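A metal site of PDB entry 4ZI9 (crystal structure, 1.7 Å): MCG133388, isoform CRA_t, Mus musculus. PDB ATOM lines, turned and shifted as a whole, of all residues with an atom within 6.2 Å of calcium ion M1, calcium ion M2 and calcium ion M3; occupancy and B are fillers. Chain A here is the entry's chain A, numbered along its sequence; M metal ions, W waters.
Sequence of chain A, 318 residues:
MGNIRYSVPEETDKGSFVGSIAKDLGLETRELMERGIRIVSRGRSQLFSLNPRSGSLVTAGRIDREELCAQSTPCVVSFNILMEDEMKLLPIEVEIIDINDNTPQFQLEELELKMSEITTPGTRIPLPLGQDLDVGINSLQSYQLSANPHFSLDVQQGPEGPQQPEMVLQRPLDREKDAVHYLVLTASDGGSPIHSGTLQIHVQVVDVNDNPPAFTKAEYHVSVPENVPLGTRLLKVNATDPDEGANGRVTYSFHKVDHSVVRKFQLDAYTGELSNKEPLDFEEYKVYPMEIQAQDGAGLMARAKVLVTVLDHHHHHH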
ATOM      1  N   GLU A  10     -17.746 -18.437  12.890  1.00  0.00           N
ATOM      2  CA  GLU A  10     -17.692 -19.538  11.938  1.00  0.00           C
ATOM      3  C   GLU A  10     -16.713 -20.617  12.429  1.00  0.00           C
ATOM      4  O   GLU A  10     -15.876 -20.366  13.282  1.00  0.00           O
ATOM      5  CB  GLU A  10     -17.237 -19.024  10.571  1.00  0.00           C
ATOM      6  CG  GLU A  10     -15.903 -18.329  10.698  1.00  0.00           C
ATOM      7  CD  GLU A  10     -15.243 -18.038   9.372  1.00  0.00           C
ATOM      8  OE1 GLU A  10     -15.480 -18.775   8.391  1.00  0.00           O
ATOM      9  OE2 GLU A  10     -14.476 -17.059   9.319  1.00  0.00           O
ATOM     10  N   GLU A  11     -16.855 -21.816  11.878  1.00  0.00           N
ATOM     11  CA  GLU A  11     -15.934 -22.941  12.073  1.00  0.00           C
ATOM     12  C   GLU A  11     -15.850 -23.509  13.500  1.00  0.00           C
ATOM     13  O   GLU A  11     -14.899 -24.196  13.832  1.00  0.00           O
ATOM     14  CB  GLU A  11     -14.508 -22.541  11.595  1.00  0.00           C
ATOM     15  CG  GLU A  11     -14.467 -21.825  10.221  1.00  0.00           C
ATOM     16  CD  GLU A  11     -14.725 -22.730   9.026  1.00  0.00           C
ATOM     17  OE1 GLU A  11     -15.023 -23.927   9.222  1.00  0.00           O
ATOM     18  OE2 GLU A  11     -14.606 -22.241   7.879  1.00  0.00           O
ATOM     19  N   ARG A  62     -20.926 -27.720   9.789  1.00  0.00           N
ATOM     20  CA  ARG A  62     -19.869 -26.749   9.541  1.00  0.00           C
ATOM     21  C   ARG A  62     -20.491 -25.415   9.117  1.00  0.00           C
ATOM     22  O   ARG A  62     -21.281 -25.367   8.186  1.00  0.00           O
ATOM     23  CB  ARG A  62     -18.875 -27.221   8.466  1.00  0.00           C
ATOM     24  CG  ARG A  62     -17.679 -26.271   8.339  1.00  0.00           C
ATOM     25  CD  ARG A  62     -16.713 -26.565   7.169  1.00  0.00           C
ATOM     26  NE  ARG A  62     -15.720 -25.497   7.084  1.00  0.00           N
ATOM     27  CZ  ARG A  62     -14.971 -25.222   6.014  1.00  0.00           C
ATOM     28  NH1 ARG A  62     -15.085 -25.957   4.906  1.00  0.00           N
ATOM     29  NH2 ARG A  62     -14.105 -24.219   6.025  1.00  0.00           N
ATOM     30  N   ILE A  63     -20.153 -24.344   9.824  1.00  0.00           N
ATOM     31  CA  ILE A  63     -20.541 -23.009   9.370  1.00  0.00           C
ATOM     32  C   ILE A  63     -19.300 -22.256   8.870  1.00  0.00           C
ATOM     33  O   ILE A  63     -18.423 -21.868   9.653  1.00  0.00           O
ATOM     34  CB  ILE A  63     -21.254 -22.205  10.492  1.00  0.00           C
ATOM     35  CG1 ILE A  63     -22.353 -23.061  11.143  1.00  0.00           C
ATOM     36  CG2 ILE A  63     -21.825 -20.905   9.904  1.00  0.00           C
ATOM     37  CD1 ILE A  63     -23.078 -22.399  12.298  1.00  0.00           C
ATOM     38  N   ASP A  64     -19.221 -22.072   7.554  1.00  0.00           N
ATOM     39  CA  ASP A  64     -18.101 -21.375   6.935  1.00  0.00           C
ATOM     40  C   ASP A  64     -18.587 -20.041   6.382  1.00  0.00           C
ATOM     41  O   ASP A  64     -19.309 -20.004   5.395  1.00  0.00           O
ATOM     42  CB  ASP A  64     -17.488 -22.225   5.820  1.00  0.00           C
ATOM     43  CG  ASP A  64     -16.421 -21.482   4.999  1.00  0.00           C
ATOM     44  OD1 ASP A  64     -15.755 -20.548   5.513  1.00  0.00           O
ATOM     45  OD2 ASP A  64     -16.258 -21.826   3.814  1.00  0.00           O
ATOM     46  N   ARG A  65     -18.190 -18.939   7.027  1.00  0.00           N
ATOM     47  CA  ARG A  65     -18.609 -17.593   6.621  1.00  0.00           C
ATOM     48  C   ARG A  65     -18.222 -17.273   5.182  1.00  0.00           C
ATOM     49  O   ARG A  65     -18.939 -16.572   4.472  1.00  0.00           O
ATOM     50  CB  ARG A  65     -18.025 -16.530   7.564  1.00  0.00           C
ATOM     51  CG  ARG A  65     -18.693 -15.152   7.396  1.00  0.00           C
ATOM     52  CD  ARG A  65     -17.725 -14.031   7.658  1.00  0.00           C
ATOM     53  NE  ARG A  65     -16.641 -14.080   6.671  1.00  0.00           N
ATOM     54  CZ  ARG A  65     -16.761 -13.662   5.424  1.00  0.00           C
ATOM     55  NH1 ARG A  65     -17.905 -13.135   5.001  1.00  0.00           N
ATOM     56  NH2 ARG A  65     -15.723 -13.782   4.592  1.00  0.00           N
ATOM     57  N   GLU A  66     -17.082 -17.791   4.754  1.00  0.00           N
ATOM     58  CA  GLU A  66     -16.634 -17.515   3.399  1.00  0.00           C
ATOM     59  C   GLU A  66     -17.611 -18.126   2.396  1.00  0.00           C
ATOM     60  O   GLU A  66     -18.031 -17.468   1.452  1.00  0.00           O
ATOM     61  CB  GLU A  66     -15.206 -18.040   3.176  1.00  0.00           C
ATOM     62  CG  GLU A  66     -14.116 -17.090   3.679  1.00  0.00           C
ATOM     63  CD  GLU A  66     -14.029 -16.949   5.192  1.00  0.00           C
ATOM     64  OE1 GLU A  66     -13.783 -17.928   5.916  1.00  0.00           O
ATOM     65  OE2 GLU A  66     -14.142 -15.806   5.678  1.00  0.00           O
ATOM     66  N   GLU A  67     -18.015 -19.371   2.640  1.00  0.00           N
ATOM     67  CA  GLU A  67     -18.977 -20.014   1.752  1.00  0.00           C
ATOM     68  C   GLU A  67     -20.349 -19.331   1.760  1.00  0.00           C
ATOM     69  O   GLU A  67     -20.999 -19.220   0.715  1.00  0.00           O
ATOM     70  CB  GLU A  67     -19.144 -21.484   2.122  1.00  0.00           C
ATOM     71  CG  GLU A  67     -20.154 -22.206   1.239  1.00  0.00           C
ATOM     72  CD  GLU A  67     -20.540 -23.572   1.786  1.00  0.00           C
ATOM     73  OE1 GLU A  67     -19.727 -24.167   2.528  1.00  0.00           O
ATOM     74  OE2 GLU A  67     -21.663 -24.039   1.480  1.00  0.00           O
ATOM     75  N   ASP A  98     -16.707 -13.459  11.401  1.00  0.00           N
ATOM     76  CA  ASP A  98     -15.551 -13.851  10.599  1.00  0.00           C
ATOM     77  C   ASP A  98     -14.379 -14.197  11.490  1.00  0.00           C
ATOM     78  O   ASP A  98     -14.113 -13.494  12.458  1.00  0.00           O
ATOM     79  CB  ASP A  98     -15.148 -12.716   9.647  1.00  0.00           C
ATOM     80  CG  ASP A  98     -14.003 -13.090   8.729  1.00  0.00           C
ATOM     81  OD1 ASP A  98     -14.058 -14.156   8.083  1.00  0.00           O
ATOM     82  OD2 ASP A  98     -13.050 -12.281   8.607  1.00  0.00           O
ATOM     83  N   ILE A  99     -13.676 -15.282  11.192  1.00  0.00           N
ATOM     84  CA  ILE A  99     -12.392 -15.471  11.835  1.00  0.00           C
ATOM     85  C   ILE A  99     -11.345 -15.436  10.733  1.00  0.00           C
ATOM     86  O   ILE A  99     -11.653 -15.579   9.538  1.00  0.00           O
ATOM     87  CB  ILE A  99     -12.281 -16.792  12.598  1.00  0.00           C
ATOM     88  CG1 ILE A  99     -12.195 -17.956  11.623  1.00  0.00           C
ATOM     89  CG2 ILE A  99     -13.477 -16.962  13.561  1.00  0.00           C
ATOM     90  CD1 ILE A  99     -11.910 -19.285  12.296  1.00  0.00           C
ATOM     91  N   ASN A 100     -10.108 -15.250  11.156  1.00  0.00           N
ATOM     92  CA  ASN A 100      -9.027 -15.133  10.194  1.00  0.00           C
ATOM     93  C   ASN A 100      -8.497 -16.492   9.826  1.00  0.00           C
ATOM     94  O   ASN A 100      -7.407 -16.858  10.258  1.00  0.00           O
ATOM     95  CB  ASN A 100      -7.903 -14.261  10.767  1.00  0.00           C
ATOM     96  CG  ASN A 100      -6.949 -13.799   9.670  1.00  0.00           C
ATOM     97  OD1 ASN A 100      -7.370 -13.667   8.532  1.00  0.00           O
ATOM     98  ND2 ASN A 100      -5.692 -13.552  10.015  1.00  0.00           N
ATOM     99  N   ASP A 101      -9.237 -17.251   9.016  1.00  0.00           N
ATOM    100  CA  ASP A 101      -8.790 -18.590   8.640  1.00  0.00           C
ATOM    101  C   ASP A 101      -8.368 -18.689   7.163  1.00  0.00           C
ATOM    102  O   ASP A 101      -8.358 -19.775   6.583  1.00  0.00           O
ATOM    103  CB  ASP A 101      -9.872 -19.646   8.931  1.00  0.00           C
ATOM    104  CG  ASP A 101     -11.252 -19.273   8.404  1.00  0.00           C
ATOM    105  OD1 ASP A 101     -11.486 -18.075   8.131  1.00  0.00           O
ATOM    106  OD2 ASP A 101     -12.115 -20.169   8.286  1.00  0.00           O
ATOM    107  N   ASN A 102      -8.060 -17.545   6.568  1.00  0.00           N
ATOM    108  CA  ASN A 102      -7.580 -17.529   5.195  1.00  0.00           C
ATOM    109  C   ASN A 102      -6.358 -16.645   5.086  1.00  0.00           C
ATOM    110  O   ASN A 102      -6.278 -15.607   5.732  1.00  0.00           O
ATOM    111  CB  ASN A 102      -8.658 -17.055   4.233  1.00  0.00           C
ATOM    112  CG  ASN A 102      -9.774 -18.059   4.091  1.00  0.00           C
ATOM    113  OD1 ASN A 102      -9.695 -18.989   3.278  1.00  0.00           O
ATOM    114  ND2 ASN A 102     -10.827 -17.884   4.882  1.00  0.00           N
ATOM    115  N   THR A 103      -5.383 -17.100   4.301  1.00  0.00           N
ATOM    116  CA  THR A 103      -4.187 -16.326   3.981  1.00  0.00           C
ATOM    117  C   THR A 103      -4.351 -15.645   2.625  1.00  0.00           C
ATOM    118  O   THR A 103      -4.903 -16.255   1.686  1.00  0.00           O
ATOM    119  CB  THR A 103      -2.958 -17.248   3.987  1.00  0.00           C
ATOM    120  OG1 THR A 103      -2.827 -17.843   5.280  1.00  0.00           O
ATOM    121  CG2 THR A 103      -1.674 -16.492   3.618  1.00  0.00           C
ATOM    122  N   PRO A 104      -3.877 -14.395   2.482  1.00  0.00           N
ATOM    123  CA  PRO A 104      -3.915 -13.786   1.143  1.00  0.00           C
ATOM    124  C   PRO A 104      -3.233 -14.685   0.102  1.00  0.00           C
ATOM    125  O   PRO A 104      -2.146 -15.190   0.324  1.00  0.00           O
ATOM    126  CB  PRO A 104      -3.143 -12.469   1.330  1.00  0.00           C
ATOM    127  CG  PRO A 104      -3.270 -12.162   2.780  1.00  0.00           C
ATOM    128  CD  PRO A 104      -3.298 -13.485   3.492  1.00  0.00           C
ATOM    129  N   ASP A 132      -7.547 -12.018  -0.257  1.00  0.00           N
ATOM    130  CA  ASP A 132      -7.866 -12.692   1.003  1.00  0.00           C
ATOM    131  C   ASP A 132      -9.373 -12.944   1.117  1.00  0.00           C
ATOM    132  O   ASP A 132     -10.164 -12.018   0.984  1.00  0.00           O
ATOM    133  CB  ASP A 132      -7.386 -11.820   2.170  1.00  0.00           C
ATOM    134  CG  ASP A 132      -7.320 -12.571   3.493  1.00  0.00           C
ATOM    135  OD1 ASP A 132      -8.330 -13.187   3.908  1.00  0.00           O
ATOM    136  OD2 ASP A 132      -6.256 -12.550   4.120  1.00  0.00           O
ATOM    137  N   LEU A 133      -9.779 -14.198   1.338  1.00  0.00           N
ATOM    138  CA  LEU A 133     -11.200 -14.568   1.387  1.00  0.00           C
ATOM    139  C   LEU A 133     -11.931 -14.067   2.621  1.00  0.00           C
ATOM    140  O   LEU A 133     -13.169 -14.023   2.655  1.00  0.00           O
ATOM    141  CB  LEU A 133     -11.358 -16.075   1.301  1.00  0.00           C
ATOM    142  CG  LEU A 133     -10.912 -16.681  -0.026  1.00  0.00           C
ATOM    143  CD1 LEU A 133     -11.115 -18.191  -0.005  1.00  0.00           C
ATOM    144  CD2 LEU A 133     -11.687 -16.043  -1.170  1.00  0.00           C
ATOM    145  N   ASP A 134     -11.170 -13.716   3.653  1.00  0.00           N
ATOM    146  CA  ASP A 134     -11.767 -13.170   4.873  1.00  0.00           C
ATOM    147  C   ASP A 134     -12.275 -11.753   4.621  1.00  0.00           C
ATOM    148  O   ASP A 134     -12.202 -11.235   3.499  1.00  0.00           O
ATOM    149  CB  ASP A 134     -10.765 -13.202   6.013  1.00  0.00           C
ATOM    150  CG  ASP A 134     -10.281 -14.606   6.308  1.00  0.00           C
ATOM    151  OD1 ASP A 134     -11.097 -15.552   6.270  1.00  0.00           O
ATOM    152  OD2 ASP A 134      -9.081 -14.770   6.608  1.00  0.00           O
ATOM    153  N   VAL A 135     -12.840 -11.119   5.646  1.00  0.00           N
ATOM    154  CA  VAL A 135     -13.363  -9.783   5.483  1.00  0.00           C
ATOM    155  C   VAL A 135     -12.836  -8.855   6.553  1.00  0.00           C
ATOM    156  O   VAL A 135     -12.255  -9.305   7.541  1.00  0.00           O
ATOM    157  CB  VAL A 135     -14.897  -9.757   5.515  1.00  0.00           C
ATOM    158  CG1 VAL A 135     -15.442 -10.412   4.259  1.00  0.00           C
ATOM    159  CG2 VAL A 135     -15.415 -10.464   6.769  1.00  0.00           C
ATOM    160  N   ASN A 138      -9.445  -8.844   8.707  1.00  0.00           N
ATOM    161  CA  ASN A 138      -8.852 -10.125   8.351  1.00  0.00           C
ATOM    162  C   ASN A 138      -8.531 -10.226   6.868  1.00  0.00           C
ATOM    163  O   ASN A 138      -7.982 -11.243   6.420  1.00  0.00           O
ATOM    164  CB  ASN A 138      -9.770 -11.268   8.763  1.00  0.00           C
ATOM    165  CG  ASN A 138      -9.946 -11.344  10.255  1.00  0.00           C
ATOM    166  OD1 ASN A 138      -9.005 -11.046  11.008  1.00  0.00           O
ATOM    167  ND2 ASN A 138     -11.147 -11.717  10.703  1.00  0.00           N
ATOM    168  N   SER A 139      -8.874  -9.210   6.096  1.00  0.00           N
ATOM    169  CA  SER A 139      -8.504  -9.246   4.684  1.00  0.00           C
ATOM    170  C   SER A 139      -7.165  -8.544   4.434  1.00  0.00           C
ATOM    171  O   SER A 139      -6.479  -8.086   5.364  1.00  0.00           O
ATOM    172  CB  SER A 139      -9.613  -8.631   3.812  1.00  0.00           C
ATOM    173  OG  SER A 139      -9.942  -7.337   4.259  1.00  0.00           O
ATOM    174  N   LEU A 140      -6.801  -8.476   3.159  1.00  0.00           N
ATOM    175  CA  LEU A 140      -5.520  -7.912   2.730  1.00  0.00           C
ATOM    176  C   LEU A 140      -5.319  -6.514   3.314  1.00  0.00           C
ATOM    177  O   LEU A 140      -6.185  -5.663   3.187  1.00  0.00           O
ATOM    178  CB  LEU A 140      -5.456  -7.856   1.210  1.00  0.00           C
ATOM    179  CG  LEU A 140      -4.154  -7.323   0.585  1.00  0.00           C
ATOM    180  CD1 LEU A 140      -3.014  -8.232   0.925  1.00  0.00           C
ATOM    181  CD2 LEU A 140      -4.303  -7.215  -0.919  1.00  0.00           C
ATOM    182  N   ASP A 189      -2.423 -10.011   5.792  1.00  0.00           N
ATOM    183  CA  ASP A 189      -3.704  -9.473   6.209  1.00  0.00           C
ATOM    184  C   ASP A 189      -3.502  -8.740   7.533  1.00  0.00           C
ATOM    185  O   ASP A 189      -2.370  -8.535   7.955  1.00  0.00           O
ATOM    186  CB  ASP A 189      -4.779 -10.573   6.328  1.00  0.00           C
ATOM    187  CG  ASP A 189      -4.421 -11.696   7.310  1.00  0.00           C
ATOM    188  OD1 ASP A 189      -3.666 -11.462   8.283  1.00  0.00           O
ATOM    189  OD2 ASP A 189      -4.935 -12.820   7.111  1.00  0.00           O
ATOM    190  N   GLY A 190      -4.586  -8.359   8.205  1.00  0.00           N
ATOM    191  CA  GLY A 190      -4.437  -7.617   9.439  1.00  0.00           C
ATOM    192  C   GLY A 190      -4.875  -8.361  10.689  1.00  0.00           C
ATOM    193  O   GLY A 190      -5.214  -7.752  11.709  1.00  0.00           O
ATOM    194  N   GLY A 191      -4.856  -9.700  10.630  1.00  0.00           N
ATOM    195  CA  GLY A 191      -5.252 -10.511  11.770  1.00  0.00           C
ATOM    196  C   GLY A 191      -4.164 -10.518  12.830  1.00  0.00           C
ATOM    197  O   GLY A 191      -3.152  -9.830  12.690  1.00  0.00           O
ATOM    198  N   HIS A 195      -1.424 -13.326   8.769  1.00  0.00           N
ATOM    199  CA  HIS A 195      -1.149 -14.310   7.727  1.00  0.00           C
ATOM    200  C   HIS A 195      -0.540 -13.590   6.538  1.00  0.00           C
ATOM    201  O   HIS A 195      -0.979 -12.495   6.203  1.00  0.00           O
ATOM    202  CB  HIS A 195      -2.416 -15.033   7.297  1.00  0.00           C
ATOM    203  CG  HIS A 195      -2.983 -15.913   8.367  1.00  0.00           C
ATOM    204  ND1 HIS A 195      -4.074 -16.724   8.167  1.00  0.00           N
ATOM    205  CD2 HIS A 195      -2.592 -16.101   9.653  1.00  0.00           C
ATOM    206  CE1 HIS A 195      -4.346 -17.373   9.285  1.00  0.00           C
ATOM    207  NE2 HIS A 195      -3.468 -17.014  10.202  1.00  0.00           N
HETATM  208 CA    CA M   1     -12.971 -16.307   7.619  1.00  0.00          CA
HETATM  209 CA    CA M   2      -7.061 -13.450   6.249  1.00  0.00          CA
HETATM  210 CA    CA M   3     -14.079 -20.039   6.916  1.00  0.00          CA
HETATM  211  O   HOH W   1     -12.364 -20.914   5.282  1.00  0.00           O
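Calcium ion M3 is bound by the side-chain carboxylate of Asp 64, the side-chain carboxylate of Glu 66, the side-chain carboxylate of Glu 10, the side-chain carboxylate of Asp 101, the side-chain carboxylate of Glu 11 and water W1.
Of the 26 residues printed, 5 come within 4 Å of calcium ion M3.
Calcium ion M2 is bound by the side-chain amide oxygen (OD1) of Asn 100, 2.3 Å away. Calcium ion M2 is bound by O of Asn 102 (2.4 Å). OD2 of Asp 189 binds calcium ion M2, at 2.4 Å. The backbone carbonyl oxygen (O) of Asn 138 is bound to calcium ion M2 (2.4 Å). OD2 of Asp 134 binds calcium ion M2, 2.4 Å away. OD2 of Asp 132 binds calcium ion M2 (2.4 Å). Calcium ion M2 is bound by OD1 of Asp 132. Calcium ion M2 has seven donor atoms within binding distance.
OD1 of Asp 98 sits close to NE of Arg 65 (2.9 Å). NH2 of Arg 62 lies within salt-bridge range of OD2 of Asp 64 (3.9 Å). N of Asp 189 sits at hydrogen-bond distance from O of His 195, at 2.9 Å. ND2 of Asn 102 sits close to OD1 of Asp 101 (3.3 Å). OD1 of Asp 189 sits at hydrogen-bond distance from N of Gly 191, at 3.2 Å. The side-chain carboxylate (OE1) of Glu 11 is in salt-bridge range of the guanidinium group (NE) of Arg 62 (2.7 Å). The backbone NH (N) of Glu 67 lies within hydrogen-bond range of the side-chain carboxylate (OD2) of Asp 64 (3.2 Å). A ring nitrogen (ND1) of His 195 sits close to the backbone carbonyl oxygen (O) of Asn 102 (3.5 Å).
Of the 26 residues printed, 7 come within 4 Å of calcium ion M1.
Calcium ion M1 is bound by the side-chain carboxylate (OE2) of Glu 66 (2.3 Å), the side-chain carboxylate (OD1) of Asp 101 (2.4 Å), the side-chain carboxylate (OE2) of Glu 10 (2.4 Å), the side-chain carboxylate (OD1) of Asp 134 (2.4 Å), the backbone carbonyl oxygen (O) of Ile 99 (2.4 Å), the side-chain carboxylate (OD1) of Asp 98 (2.5 Å) and the side-chain carboxylate (OE1) of Glu 66 (2.5 Å).
Six residues have an atom within 4 Å of calcium ion M2: Asn 100, Asn 102, Asp 132, Asp 134, Asn 138 and Asp 189. Along chain A the residues within 4 Å of calcium ion M2 span positions 100 to 189.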
